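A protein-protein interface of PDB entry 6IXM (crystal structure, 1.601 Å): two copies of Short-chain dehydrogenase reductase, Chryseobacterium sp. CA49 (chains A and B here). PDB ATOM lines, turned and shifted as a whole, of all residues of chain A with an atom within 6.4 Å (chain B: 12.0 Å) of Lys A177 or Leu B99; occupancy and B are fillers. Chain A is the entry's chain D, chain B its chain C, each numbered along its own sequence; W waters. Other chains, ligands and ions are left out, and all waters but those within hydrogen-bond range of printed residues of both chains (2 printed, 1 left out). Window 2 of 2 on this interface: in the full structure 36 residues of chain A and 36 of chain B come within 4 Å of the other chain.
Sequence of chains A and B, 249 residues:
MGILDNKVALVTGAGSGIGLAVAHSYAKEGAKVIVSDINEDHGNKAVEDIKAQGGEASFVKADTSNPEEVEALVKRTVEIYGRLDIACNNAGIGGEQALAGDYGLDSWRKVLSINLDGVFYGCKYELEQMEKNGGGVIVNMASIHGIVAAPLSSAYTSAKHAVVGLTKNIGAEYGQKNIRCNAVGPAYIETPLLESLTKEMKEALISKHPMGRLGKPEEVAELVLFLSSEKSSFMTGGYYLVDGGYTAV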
ATOM      1  N   LYS A 124       4.225  20.930 -31.396  1.00  0.00           N
ATOM      2  CA  LYS A 124       4.296  20.586 -29.982  1.00  0.00           C
ATOM      3  C   LYS A 124       3.198  19.600 -29.605  1.00  0.00           C
ATOM      4  O   LYS A 124       3.475  18.530 -29.053  1.00  0.00           O
ATOM      5  CB  LYS A 124       4.202  21.852 -29.129  1.00  0.00           C
ATOM      6  CG  LYS A 124       4.316  21.576 -27.624  1.00  0.00           C
ATOM      7  CD  LYS A 124       4.139  22.864 -26.834  1.00  0.00           C
ATOM      8  CE  LYS A 124       3.829  22.559 -25.386  1.00  0.00           C
ATOM      9  NZ  LYS A 124       4.885  21.708 -24.804  1.00  0.00           N
ATOM     10  N   LEU A 127       3.430  16.194 -31.606  1.00  0.00           N
ATOM     11  CA  LEU A 127       4.457  15.309 -31.065  1.00  0.00           C
ATOM     12  C   LEU A 127       3.990  14.656 -29.772  1.00  0.00           C
ATOM     13  O   LEU A 127       4.182  13.449 -29.579  1.00  0.00           O
ATOM     14  CB  LEU A 127       5.753  16.083 -30.823  1.00  0.00           C
ATOM     15  CG  LEU A 127       6.492  16.523 -32.087  1.00  0.00           C
ATOM     16  CD1 LEU A 127       7.527  17.603 -31.744  1.00  0.00           C
ATOM     17  CD2 LEU A 127       7.144  15.337 -32.811  1.00  0.00           C
ATOM     18  N   MET A 130       1.694  11.915 -30.798  1.00  0.00           N
ATOM     19  CA  MET A 130       2.337  10.850 -31.560  1.00  0.00           C
ATOM     20  C   MET A 130       3.147   9.931 -30.652  1.00  0.00           C
ATOM     21  O   MET A 130       3.181   8.713 -30.861  1.00  0.00           O
ATOM     22  CB  MET A 130       3.212  11.449 -32.661  1.00  0.00           C
ATOM     23  CG  MET A 130       2.368  11.967 -33.817  1.00  0.00           C
ATOM     24  SD  MET A 130       3.355  12.854 -35.025  1.00  0.00           S
ATOM     25  CE  MET A 130       2.105  13.105 -36.287  1.00  0.00           C
ATOM     26  N   GLU A 131       3.786  10.490 -29.621  1.00  0.00           N
ATOM     27  CA  GLU A 131       4.521   9.656 -28.677  1.00  0.00           C
ATOM     28  C   GLU A 131       3.602   8.713 -27.921  1.00  0.00           C
ATOM     29  O   GLU A 131       4.060   7.662 -27.465  1.00  0.00           O
ATOM     30  CB  GLU A 131       5.295  10.535 -27.704  1.00  0.00           C
ATOM     31  CG  GLU A 131       6.398  11.313 -28.399  1.00  0.00           C
ATOM     32  CD  GLU A 131       7.579  11.607 -27.503  1.00  0.00           C
ATOM     33  OE1 GLU A 131       7.551  12.639 -26.806  1.00  0.00           O
ATOM     34  OE2 GLU A 131       8.537  10.811 -27.505  1.00  0.00           O
ATOM     35  N   GLY A 134       2.655   5.449 -30.801  1.00  0.00           N
ATOM     36  CA  GLY A 134       3.642   4.705 -31.563  1.00  0.00           C
ATOM     37  C   GLY A 134       4.434   5.493 -32.586  1.00  0.00           C
ATOM     38  O   GLY A 134       5.199   4.892 -33.351  1.00  0.00           O
ATOM     39  N   GLY A 135       4.280   6.806 -32.635  1.00  0.00           N
ATOM     40  CA  GLY A 135       5.029   7.626 -33.569  1.00  0.00           C
ATOM     41  C   GLY A 135       4.115   8.274 -34.590  1.00  0.00           C
ATOM     42  O   GLY A 135       2.889   8.286 -34.450  1.00  0.00           O
ATOM     43  N   GLY A 136       4.730   8.814 -35.637  1.00  0.00           N
ATOM     44  CA  GLY A 136       3.969   9.540 -36.636  1.00  0.00           C
ATOM     45  C   GLY A 136       4.886  10.343 -37.539  1.00  0.00           C
ATOM     46  O   GLY A 136       6.106  10.243 -37.460  1.00  0.00           O
ATOM     47  N   GLU A 173      15.916  15.566 -33.194  1.00  0.00           N
ATOM     48  CA  GLU A 173      15.550  15.183 -31.830  1.00  0.00           C
ATOM     49  C   GLU A 173      14.776  13.875 -31.791  1.00  0.00           C
ATOM     50  O   GLU A 173      14.903  13.105 -30.831  1.00  0.00           O
ATOM     51  CB  GLU A 173      14.706  16.273 -31.184  1.00  0.00           C
ATOM     52  CG  GLU A 173      15.503  17.489 -30.716  1.00  0.00           C
ATOM     53  CD  GLU A 173      14.609  18.621 -30.264  1.00  0.00           C
ATOM     54  OE1 GLU A 173      13.394  18.403 -30.132  1.00  0.00           O
ATOM     55  OE2 GLU A 173      15.127  19.735 -30.044  1.00  0.00           O
ATOM     56  N   TYR A 174      13.929  13.624 -32.793  1.00  0.00           N
ATOM     57  CA  TYR A 174      12.992  12.509 -32.730  1.00  0.00           C
ATOM     58  C   TYR A 174      13.387  11.347 -33.640  1.00  0.00           C
ATOM     59  O   TYR A 174      12.582  10.434 -33.851  1.00  0.00           O
ATOM     60  CB  TYR A 174      11.577  13.012 -33.041  1.00  0.00           C
ATOM     61  CG  TYR A 174      11.007  13.826 -31.884  1.00  0.00           C
ATOM     62  CD1 TYR A 174      11.327  15.171 -31.715  1.00  0.00           C
ATOM     63  CD2 TYR A 174      10.190  13.223 -30.926  1.00  0.00           C
ATOM     64  CE1 TYR A 174      10.830  15.900 -30.644  1.00  0.00           C
ATOM     65  CE2 TYR A 174       9.690  13.935 -29.853  1.00  0.00           C
ATOM     66  CZ  TYR A 174      10.004  15.275 -29.712  1.00  0.00           C
ATOM     67  OH  TYR A 174       9.506  15.974 -28.634  1.00  0.00           O
ATOM     68  N   GLY A 175      14.625  11.347 -34.144  1.00  0.00           N
ATOM     69  CA  GLY A 175      15.045  10.349 -35.113  1.00  0.00           C
ATOM     70  C   GLY A 175      14.902   8.923 -34.625  1.00  0.00           C
ATOM     71  O   GLY A 175      14.613   8.023 -35.414  1.00  0.00           O
ATOM     72  N   GLN A 176      15.117   8.689 -33.331  1.00  0.00           N
ATOM     73  CA  GLN A 176      14.961   7.352 -32.769  1.00  0.00           C
ATOM     74  C   GLN A 176      13.660   7.193 -31.991  1.00  0.00           C
ATOM     75  O   GLN A 176      13.526   6.254 -31.193  1.00  0.00           O
ATOM     76  CB  GLN A 176      16.171   7.005 -31.895  1.00  0.00           C
ATOM     77  CG  GLN A 176      17.457   6.880 -32.709  1.00  0.00           C
ATOM     78  CD  GLN A 176      18.668   6.522 -31.868  1.00  0.00           C
ATOM     79  OE1 GLN A 176      19.417   7.396 -31.432  1.00  0.00           O
ATOM     80  NE2 GLN A 176      18.868   5.233 -31.644  1.00  0.00           N
ATOM     81  N   LYS A 177      12.679   8.062 -32.236  1.00  0.00           N
ATOM     82  CA  LYS A 177      11.389   7.991 -31.558  1.00  0.00           C
ATOM     83  C   LYS A 177      10.245   7.684 -32.520  1.00  0.00           C
ATOM     84  O   LYS A 177       9.087   8.004 -32.221  1.00  0.00           O
ATOM     85  CB  LYS A 177      11.132   9.289 -30.787  1.00  0.00           C
ATOM     86  CG  LYS A 177      12.067   9.463 -29.584  1.00  0.00           C
ATOM     87  CD  LYS A 177      12.280  10.928 -29.246  1.00  0.00           C
ATOM     88  CE  LYS A 177      12.186  11.196 -27.760  1.00  0.00           C
ATOM     89  NZ  LYS A 177      13.194  10.468 -26.953  1.00  0.00           N
ATOM     90  N   ASN A 178      10.541   7.064 -33.667  1.00  0.00           N
ATOM     91  CA  ASN A 178       9.520   6.651 -34.636  1.00  0.00           C
ATOM     92  C   ASN A 178       8.710   7.831 -35.158  1.00  0.00           C
ATOM     93  O   ASN A 178       7.536   7.682 -35.497  1.00  0.00           O
ATOM     94  CB  ASN A 178       8.566   5.605 -34.045  1.00  0.00           C
ATOM     95  CG  ASN A 178       9.289   4.387 -33.528  1.00  0.00           C
ATOM     96  OD1 ASN A 178      10.031   3.735 -34.259  1.00  0.00           O
ATOM     97  ND2 ASN A 178       9.084   4.075 -32.251  1.00  0.00           N
ATOM     98  N   ILE A 179       9.325   9.003 -35.211  1.00  0.00           N
ATOM     99  CA  ILE A 179       8.677  10.224 -35.663  1.00  0.00           C
ATOM    100  C   ILE A 179       9.584  10.880 -36.687  1.00  0.00           C
ATOM    101  O   ILE A 179      10.803  10.937 -36.500  1.00  0.00           O
ATOM    102  CB  ILE A 179       8.392  11.177 -34.489  1.00  0.00           C
ATOM    103  CG1 ILE A 179       7.250  10.619 -33.637  1.00  0.00           C
ATOM    104  CG2 ILE A 179       8.008  12.566 -34.998  1.00  0.00           C
ATOM    105  CD1 ILE A 179       7.120  11.340 -32.308  1.00  0.00           C
ATOM    106  N   GLY B  94      19.827  31.926 -24.628  1.00  0.00           N
ATOM    107  CA  GLY B  94      19.857  30.542 -25.071  1.00  0.00           C
ATOM    108  C   GLY B  94      18.552  29.777 -24.920  1.00  0.00           C
ATOM    109  O   GLY B  94      18.261  28.881 -25.723  1.00  0.00           O
ATOM    110  N   GLY B  95      17.759  30.108 -23.902  1.00  0.00           N
ATOM    111  CA  GLY B  95      16.496  29.437 -23.660  1.00  0.00           C
ATOM    112  C   GLY B  95      16.656  28.138 -22.889  1.00  0.00           C
ATOM    113  O   GLY B  95      17.755  27.645 -22.646  1.00  0.00           O
ATOM    114  N   GLU B  96      15.521  27.564 -22.500  1.00  0.00           N
ATOM    115  CA  GLU B  96      15.582  26.281 -21.823  1.00  0.00           C
ATOM    116  C   GLU B  96      15.990  25.180 -22.802  1.00  0.00           C
ATOM    117  O   GLU B  96      15.932  25.340 -24.029  1.00  0.00           O
ATOM    118  CB  GLU B  96      14.243  25.946 -21.168  1.00  0.00           C
ATOM    119  CG  GLU B  96      13.288  25.123 -22.028  1.00  0.00           C
ATOM    120  CD  GLU B  96      11.866  25.170 -21.494  1.00  0.00           C
ATOM    121  OE1 GLU B  96      10.947  24.635 -22.148  1.00  0.00           O
ATOM    122  OE2 GLU B  96      11.669  25.751 -20.407  1.00  0.00           O
ATOM    123  N   GLN B  97      16.431  24.059 -22.247  1.00  0.00           N
ATOM    124  CA  GLN B  97      16.762  22.874 -23.025  1.00  0.00           C
ATOM    125  C   GLN B  97      15.675  21.836 -22.797  1.00  0.00           C
ATOM    126  O   GLN B  97      15.471  21.382 -21.665  1.00  0.00           O
ATOM    127  CB  GLN B  97      18.133  22.320 -22.646  1.00  0.00           C
ATOM    128  CG  GLN B  97      19.285  23.092 -23.260  1.00  0.00           C
ATOM    129  CD  GLN B  97      20.623  22.471 -22.939  1.00  0.00           C
ATOM    130  OE1 GLN B  97      21.538  23.150 -22.483  1.00  0.00           O
ATOM    131  NE2 GLN B  97      20.744  21.172 -23.173  1.00  0.00           N
ATOM    132  N   ALA B  98      14.979  21.470 -23.871  1.00  0.00           N
ATOM    133  CA  ALA B  98      13.890  20.509 -23.815  1.00  0.00           C
ATOM    134  C   ALA B  98      13.595  20.049 -25.233  1.00  0.00           C
ATOM    135  O   ALA B  98      13.853  20.774 -26.197  1.00  0.00           O
ATOM    136  CB  ALA B  98      12.624  21.114 -23.188  1.00  0.00           C
ATOM    137  N   LEU B  99      13.074  18.832 -25.348  1.00  0.00           N
ATOM    138  CA  LEU B  99      12.594  18.357 -26.636  1.00  0.00           C
ATOM    139  C   LEU B  99      11.499  19.284 -27.136  1.00  0.00           C
ATOM    140  O   LEU B  99      10.768  19.890 -26.347  1.00  0.00           O
ATOM    141  CB  LEU B  99      12.063  16.932 -26.515  1.00  0.00           C
ATOM    142  CG  LEU B  99      13.101  15.833 -26.275  1.00  0.00           C
ATOM    143  CD1 LEU B  99      12.392  14.554 -25.852  1.00  0.00           C
ATOM    144  CD2 LEU B  99      13.955  15.598 -27.518  1.00  0.00           C
ATOM    145  N   ALA B 100      11.382  19.392 -28.462  1.00  0.00           N
ATOM    146  CA  ALA B 100      10.388  20.297 -29.026  1.00  0.00           C
ATOM    147  C   ALA B 100       8.987  20.006 -28.494  1.00  0.00           C
ATOM    148  O   ALA B 100       8.226  20.929 -28.183  1.00  0.00           O
ATOM    149  CB  ALA B 100      10.409  20.205 -30.549  1.00  0.00           C
ATOM    150  N   GLY B 101       8.623  18.729 -28.388  1.00  0.00           N
ATOM    151  CA  GLY B 101       7.315  18.387 -27.863  1.00  0.00           C
ATOM    152  C   GLY B 101       7.130  18.737 -26.398  1.00  0.00           C
ATOM    153  O   GLY B 101       5.990  18.823 -25.930  1.00  0.00           O
ATOM    154  N   ASP B 102       8.224  18.951 -25.674  1.00  0.00           N
ATOM    155  CA  ASP B 102       8.189  19.336 -24.268  1.00  0.00           C
ATOM    156  C   ASP B 102       8.446  20.822 -24.053  1.00  0.00           C
ATOM    157  O   ASP B 102       8.467  21.271 -22.901  1.00  0.00           O
ATOM    158  CB  ASP B 102       9.231  18.534 -23.473  1.00  0.00           C
ATOM    159  CG  ASP B 102       8.934  17.048 -23.438  1.00  0.00           C
ATOM    160  OD1 ASP B 102       7.743  16.674 -23.401  1.00  0.00           O
ATOM    161  OD2 ASP B 102       9.900  16.254 -23.409  1.00  0.00           O
ATOM    162  N   TYR B 103       8.630  21.597 -25.123  1.00  0.00           N
ATOM    163  CA  TYR B 103       9.161  22.948 -24.983  1.00  0.00           C
ATOM    164  C   TYR B 103       8.101  23.876 -24.411  1.00  0.00           C
ATOM    165  O   TYR B 103       6.957  23.893 -24.875  1.00  0.00           O
ATOM    166  CB  TYR B 103       9.663  23.480 -26.335  1.00  0.00           C
ATOM    167  CG  TYR B 103      10.856  24.381 -26.159  1.00  0.00           C
ATOM    168  CD1 TYR B 103      12.142  23.846 -26.091  1.00  0.00           C
ATOM    169  CD2 TYR B 103      10.697  25.754 -25.989  1.00  0.00           C
ATOM    170  CE1 TYR B 103      13.246  24.662 -25.881  1.00  0.00           C
ATOM    171  CE2 TYR B 103      11.793  26.576 -25.784  1.00  0.00           C
ATOM    172  CZ  TYR B 103      13.060  26.022 -25.731  1.00  0.00           C
ATOM    173  OH  TYR B 103      14.159  26.825 -25.514  1.00  0.00           O
ATOM    174  N   GLY B 104       8.483  24.651 -23.402  1.00  0.00           N
ATOM    175  CA  GLY B 104       7.522  25.521 -22.751  1.00  0.00           C
ATOM    176  C   GLY B 104       7.059  26.633 -23.674  1.00  0.00           C
ATOM    177  O   GLY B 104       7.837  27.200 -24.441  1.00  0.00           O
ATOM    178  N   LEU B 105       5.769  26.953 -23.585  1.00  0.00           N
ATOM    179  CA  LEU B 105       5.251  28.103 -24.313  1.00  0.00           C
ATOM    180  C   LEU B 105       5.976  29.368 -23.889  1.00  0.00           C
ATOM    181  O   LEU B 105       6.311  30.209 -24.732  1.00  0.00           O
ATOM    182  CB  LEU B 105       3.752  28.253 -24.079  1.00  0.00           C
ATOM    183  CG  LEU B 105       2.877  27.088 -24.538  1.00  0.00           C
ATOM    184  CD1 LEU B 105       1.428  27.401 -24.240  1.00  0.00           C
ATOM    185  CD2 LEU B 105       3.069  26.810 -26.021  1.00  0.00           C
ATOM    186  N   ASP B 106       6.248  29.503 -22.584  1.00  0.00           N
ATOM    187  CA  ASP B 106       6.944  30.690 -22.096  1.00  0.00           C
ATOM    188  C   ASP B 106       8.356  30.779 -22.657  1.00  0.00           C
ATOM    189  O   ASP B 106       8.779  31.849 -23.107  1.00  0.00           O
ATOM    190  CB  ASP B 106       6.963  30.718 -20.560  1.00  0.00           C
ATOM    191  CG  ASP B 106       7.611  29.484 -19.929  1.00  0.00           C
ATOM    192  OD1 ASP B 106       7.742  28.433 -20.589  1.00  0.00           O
ATOM    193  OD2 ASP B 106       7.976  29.566 -18.732  1.00  0.00           O
ATOM    194  N   SER B 107       9.094  29.666 -22.677  1.00  0.00           N
ATOM    195  CA  SER B 107      10.464  29.750 -23.166  1.00  0.00           C
ATOM    196  C   SER B 107      10.499  29.984 -24.671  1.00  0.00           C
ATOM    197  O   SER B 107      11.343  30.741 -25.161  1.00  0.00           O
ATOM    198  CB  SER B 107      11.258  28.500 -22.790  1.00  0.00           C
ATOM    199  OG  SER B 107      12.647  28.747 -22.973  1.00  0.00           O
ATOM    200  N   TRP B 108       9.577  29.369 -25.421  1.00  0.00           N
ATOM    201  CA  TRP B 108       9.482  29.670 -26.848  1.00  0.00           C
ATOM    202  C   TRP B 108       9.288  31.165 -27.075  1.00  0.00           C
ATOM    203  O   TRP B 108      10.021  31.793 -27.854  1.00  0.00           O
ATOM    204  CB  TRP B 108       8.326  28.884 -27.496  1.00  0.00           C
ATOM    205  CG  TRP B 108       8.173  29.189 -28.970  1.00  0.00           C
ATOM    206  CD1 TRP B 108       7.382  30.145 -29.535  1.00  0.00           C
ATOM    207  CD2 TRP B 108       8.848  28.536 -30.048  1.00  0.00           C
ATOM    208  NE1 TRP B 108       7.530  30.136 -30.908  1.00  0.00           N
ATOM    209  CE2 TRP B 108       8.421  29.153 -31.245  1.00  0.00           C
ATOM    210  CE3 TRP B 108       9.767  27.482 -30.119  1.00  0.00           C
ATOM    211  CZ2 TRP B 108       8.884  28.752 -32.498  1.00  0.00           C
ATOM    212  CZ3 TRP B 108      10.227  27.084 -31.370  1.00  0.00           C
ATOM    213  CH2 TRP B 108       9.791  27.723 -32.536  1.00  0.00           C
ATOM    214  N   VAL B 111      12.452  33.348 -26.075  1.00  0.00           N
ATOM    215  CA  VAL B 111      13.597  33.221 -26.978  1.00  0.00           C
ATOM    216  C   VAL B 111      13.311  33.920 -28.302  1.00  0.00           C
ATOM    217  O   VAL B 111      14.156  34.645 -28.838  1.00  0.00           O
ATOM    218  CB  VAL B 111      13.958  31.739 -27.190  1.00  0.00           C
ATOM    219  CG1 VAL B 111      14.977  31.598 -28.324  1.00  0.00           C
ATOM    220  CG2 VAL B 111      14.511  31.149 -25.917  1.00  0.00           C
ATOM    221  N   ALA B 149      20.706  22.375 -36.853  1.00  0.00           N
ATOM    222  CA  ALA B 149      19.930  22.247 -35.625  1.00  0.00           C
ATOM    223  C   ALA B 149      20.810  22.218 -34.380  1.00  0.00           C
ATOM    224  O   ALA B 149      21.988  21.858 -34.425  1.00  0.00           O
ATOM    225  CB  ALA B 149      19.091  20.967 -35.666  1.00  0.00           C
ATOM    226  N   ALA B 150      20.217  22.629 -33.256  1.00  0.00           N
ATOM    227  CA  ALA B 150      20.800  22.479 -31.923  1.00  0.00           C
ATOM    228  C   ALA B 150      19.796  21.650 -31.142  1.00  0.00           C
ATOM    229  O   ALA B 150      18.848  22.208 -30.575  1.00  0.00           O
ATOM    230  CB  ALA B 150      21.036  23.828 -31.241  1.00  0.00           C
ATOM    231  N   PRO B 151      19.936  20.323 -31.123  1.00  0.00           N
ATOM    232  CA  PRO B 151      18.958  19.485 -30.420  1.00  0.00           C
ATOM    233  C   PRO B 151      18.765  19.964 -28.991  1.00  0.00           C
ATOM    234  O   PRO B 151      19.732  20.271 -28.288  1.00  0.00           O
ATOM    235  CB  PRO B 151      19.590  18.087 -30.470  1.00  0.00           C
ATOM    236  CG  PRO B 151      20.439  18.126 -31.718  1.00  0.00           C
ATOM    237  CD  PRO B 151      20.979  19.523 -31.794  1.00  0.00           C
ATOM    238  N   LEU B 152      17.495  20.064 -28.592  1.00  0.00           N
ATOM    239  CA  LEU B 152      16.963  20.545 -27.313  1.00  0.00           C
ATOM    240  C   LEU B 152      16.871  22.070 -27.257  1.00  0.00           C
ATOM    241  O   LEU B 152      16.410  22.608 -26.240  1.00  0.00           O
ATOM    242  CB  LEU B 152      17.756  20.047 -26.093  1.00  0.00           C
ATOM    243  CG  LEU B 152      17.917  18.528 -26.024  1.00  0.00           C
ATOM    244  CD1 LEU B 152      18.665  18.138 -24.748  1.00  0.00           C
ATOM    245  CD2 LEU B 152      16.558  17.847 -26.111  1.00  0.00           C
ATOM    246  N   SER B 153      17.259  22.789 -28.312  1.00  0.00           N
ATOM    247  CA  SER B 153      17.155  24.249 -28.354  1.00  0.00           C
ATOM    248  C   SER B 153      16.382  24.689 -29.591  1.00  0.00           C
ATOM    249  O   SER B 153      16.852  25.507 -30.388  1.00  0.00           O
ATOM    250  CB  SER B 153      18.534  24.911 -28.315  1.00  0.00           C
ATOM    251  OG  SER B 153      19.210  24.599 -27.097  1.00  0.00           O
ATOM    252  N   SER B 154      15.163  24.162 -29.755  1.00  0.00           N
ATOM    253  CA  SER B 154      14.433  24.412 -30.998  1.00  0.00           C
ATOM    254  C   SER B 154      14.043  25.876 -31.150  1.00  0.00           C
ATOM    255  O   SER B 154      14.025  26.387 -32.275  1.00  0.00           O
ATOM    256  CB  SER B 154      13.203  23.506 -31.081  1.00  0.00           C
ATOM    257  OG  SER B 154      12.321  23.759 -30.007  1.00  0.00           O
ATOM    258  N   ALA B 155      13.742  26.573 -30.053  1.00  0.00           N
ATOM    259  CA  ALA B 155      13.408  27.991 -30.173  1.00  0.00           C
ATOM    260  C   ALA B 155      14.615  28.803 -30.635  1.00  0.00           C
ATOM    261  O   ALA B 155      14.488  29.713 -31.465  1.00  0.00           O
ATOM    262  CB  ALA B 155      12.873  28.517 -28.836  1.00  0.00           C
ATOM    263  N   TYR B 156      15.794  28.496 -30.092  1.00  0.00           N
ATOM    264  CA  TYR B 156      17.003  29.199 -30.493  1.00  0.00           C
ATOM    265  C   TYR B 156      17.297  28.986 -31.973  1.00  0.00           C
ATOM    266  O   TYR B 156      17.579  29.939 -32.713  1.00  0.00           O
ATOM    267  CB  TYR B 156      18.161  28.709 -29.620  1.00  0.00           C
ATOM    268  CG  TYR B 156      19.451  29.458 -29.822  1.00  0.00           C
ATOM    269  CD1 TYR B 156      19.693  30.645 -29.161  1.00  0.00           C
ATOM    270  CD2 TYR B 156      20.437  28.961 -30.661  1.00  0.00           C
ATOM    271  CE1 TYR B 156      20.887  31.322 -29.334  1.00  0.00           C
ATOM    272  CE2 TYR B 156      21.625  29.627 -30.843  1.00  0.00           C
ATOM    273  CZ  TYR B 156      21.846  30.808 -30.174  1.00  0.00           C
ATOM    274  OH  TYR B 156      23.030  31.485 -30.343  1.00  0.00           O
ATOM    275  N   THR B 157      17.226  27.732 -32.422  1.00  0.00           N
ATOM    276  CA  THR B 157      17.480  27.411 -33.826  1.00  0.00           C
ATOM    277  C   THR B 157      16.495  28.120 -34.737  1.00  0.00           C
ATOM    278  O   THR B 157      16.872  28.656 -35.789  1.00  0.00           O
ATOM    279  CB  THR B 157      17.384  25.903 -34.024  1.00  0.00           C
ATOM    280  OG1 THR B 157      18.344  25.268 -33.167  1.00  0.00           O
ATOM    281  CG2 THR B 157      17.637  25.523 -35.486  1.00  0.00           C
ATOM    282  N   SER B 158      15.218  28.108 -34.357  1.00  0.00           N
ATOM    283  CA  SER B 158      14.200  28.764 -35.173  1.00  0.00           C
ATOM    284  C   SER B 158      14.455  30.269 -35.250  1.00  0.00           C
ATOM    285  O   SER B 158      14.376  30.877 -36.327  1.00  0.00           O
ATOM    286  CB  SER B 158      12.815  28.480 -34.595  1.00  0.00           C
ATOM    287  OG  SER B 158      12.539  27.072 -34.532  1.00  0.00           O
HETATM  288  O   HOH W   1      13.874  21.694 -28.672  1.00  0.00           O
HETATM  289  O   HOH W   2       4.528  18.434 -23.757  1.00  0.00           O
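No position is printed for both chains. Of the 12 pairs that touch across the chains among the printed residues, none has its exchanged pair printed and touching as well.
Of the printed residues of chain B, Lys A124 touches Gly B101 (3.3 Å), Asp B102 (3.7 Å) and Tyr B103 (3.0 Å). Met A130 touches none of the printed residues of chain B. No residue of chain B comes within 4 Å of Glu A131. No residue of chain B comes within 4 Å of Gly A134. No residue of chain B comes within 4 Å of Gly A135. Glu A173 touches four residues of chain B. Tyr A174 touches just these residues of chain B: Leu B99, Ala B100 and Gly B101. No residue of chain B comes within 4 Å of Gly A175. No residue of chain B comes within 4 Å of Gln A176. No residue of chain B comes within 4 Å of Asn A178. Of chain A, only Glu A173 (3.6 Å), Tyr A174 (3.5 Å) and Lys A177 (3.9 Å) come within 4 Å of Leu B99. Printed residues of chain A within 4 Å of Asp B102: Lys A124. Of the printed residues of chain A, Tyr B103 touches Lys A124 (3.0 Å). Of the printed residues of chain A, Pro B151 touches Glu A173. Printed residues of chain A within 4 Å of Leu B152: Glu A173 (2.8 Å). The nearest residue of chain B that does not touch Lys A177 is Asp B102 (7.1 Å). The nearest residue of chain A that does not touch Leu B99 is Glu A131 (5.3 Å).
Water W1 lies within hydrogen-bond range of the backbone carbonyl oxygen (O) of Ala B98 (2.6 Å), the side-chain carboxylate (OE2) of Glu A173 (2.7 Å), the side-chain hydroxyl (OG) of Ser B154 (2.9 Å) and the backbone NH (N) of Ala B100 (3.4 Å). Water W2 bridges O of Gly B101 (2.6 Å) and NZ of Lys A124 (3.5 Å).
The side-chain hydroxyl of Tyr B103 is in hydrogen-bond range of the backbone carbonyl oxygen of Glu B96. The backbone carbonyl oxygen of Leu B152 is in hydrogen-bond range of the backbone NH of Ala B98 (3.0 Å).
Printed residues of chain A that touch a printed residue of chain B: Lys A124, Leu A127, Glu A173, Tyr A174 and Lys A177. Hydrophobic or aromatic side chains of chain A within 4 Å of the printed part of chain B: Leu A127 and Tyr A174. Of the 26 printed residues of chain B, 7 touch a printed residue of chain A. Printed residues of chain B that touch a printed residue of chain A: Leu B99, Ala B100, Gly B101, Asp B102, Tyr B103, Pro B151 and Leu B152. Hydrophobic or aromatic side chains of chain B that line the printed part of chain A: Leu B99 and Ala B100. Among the printed residues, no Asp or Glu carboxylate lies within 4 Å of a Lys or Arg side-chain nitrogen of the other chain.
Among the printed residues, merely in contact across the chains: Tyr A174 with Leu B99 (3.5 Å), Glu A173 with Leu B99 (3.6 Å), Leu A127 with Gly B101 (3.7 Å), Lys A124 with Asp B102 (3.7 Å), Glu A173 with Pro B151 (3.8 Å), Lys A177 with Leu B99 (3.9 Å) and Tyr A174 with Ala B100 (3.9 Å).
The backbone carbonyl oxygen of Gly B101 is in hydrogen-bond range of the side-chain amino group of Lys A124. The backbone carbonyl oxygen (O) of Tyr B103 sits at hydrogen-bond distance from the side-chain amino group (NZ) of Lys A124. OH of Tyr A174 is in hydrogen-bond range of N of Gly B101 (2.9 Å). The side-chain carboxylate (OE1) of Glu A173 sits at hydrogen-bond distance from the backbone NH (N) of Ala B100 (2.8 Å). The backbone NH of Leu B152 sits at hydrogen-bond distance from the side-chain carboxylate of Glu A173 (2.8 Å).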
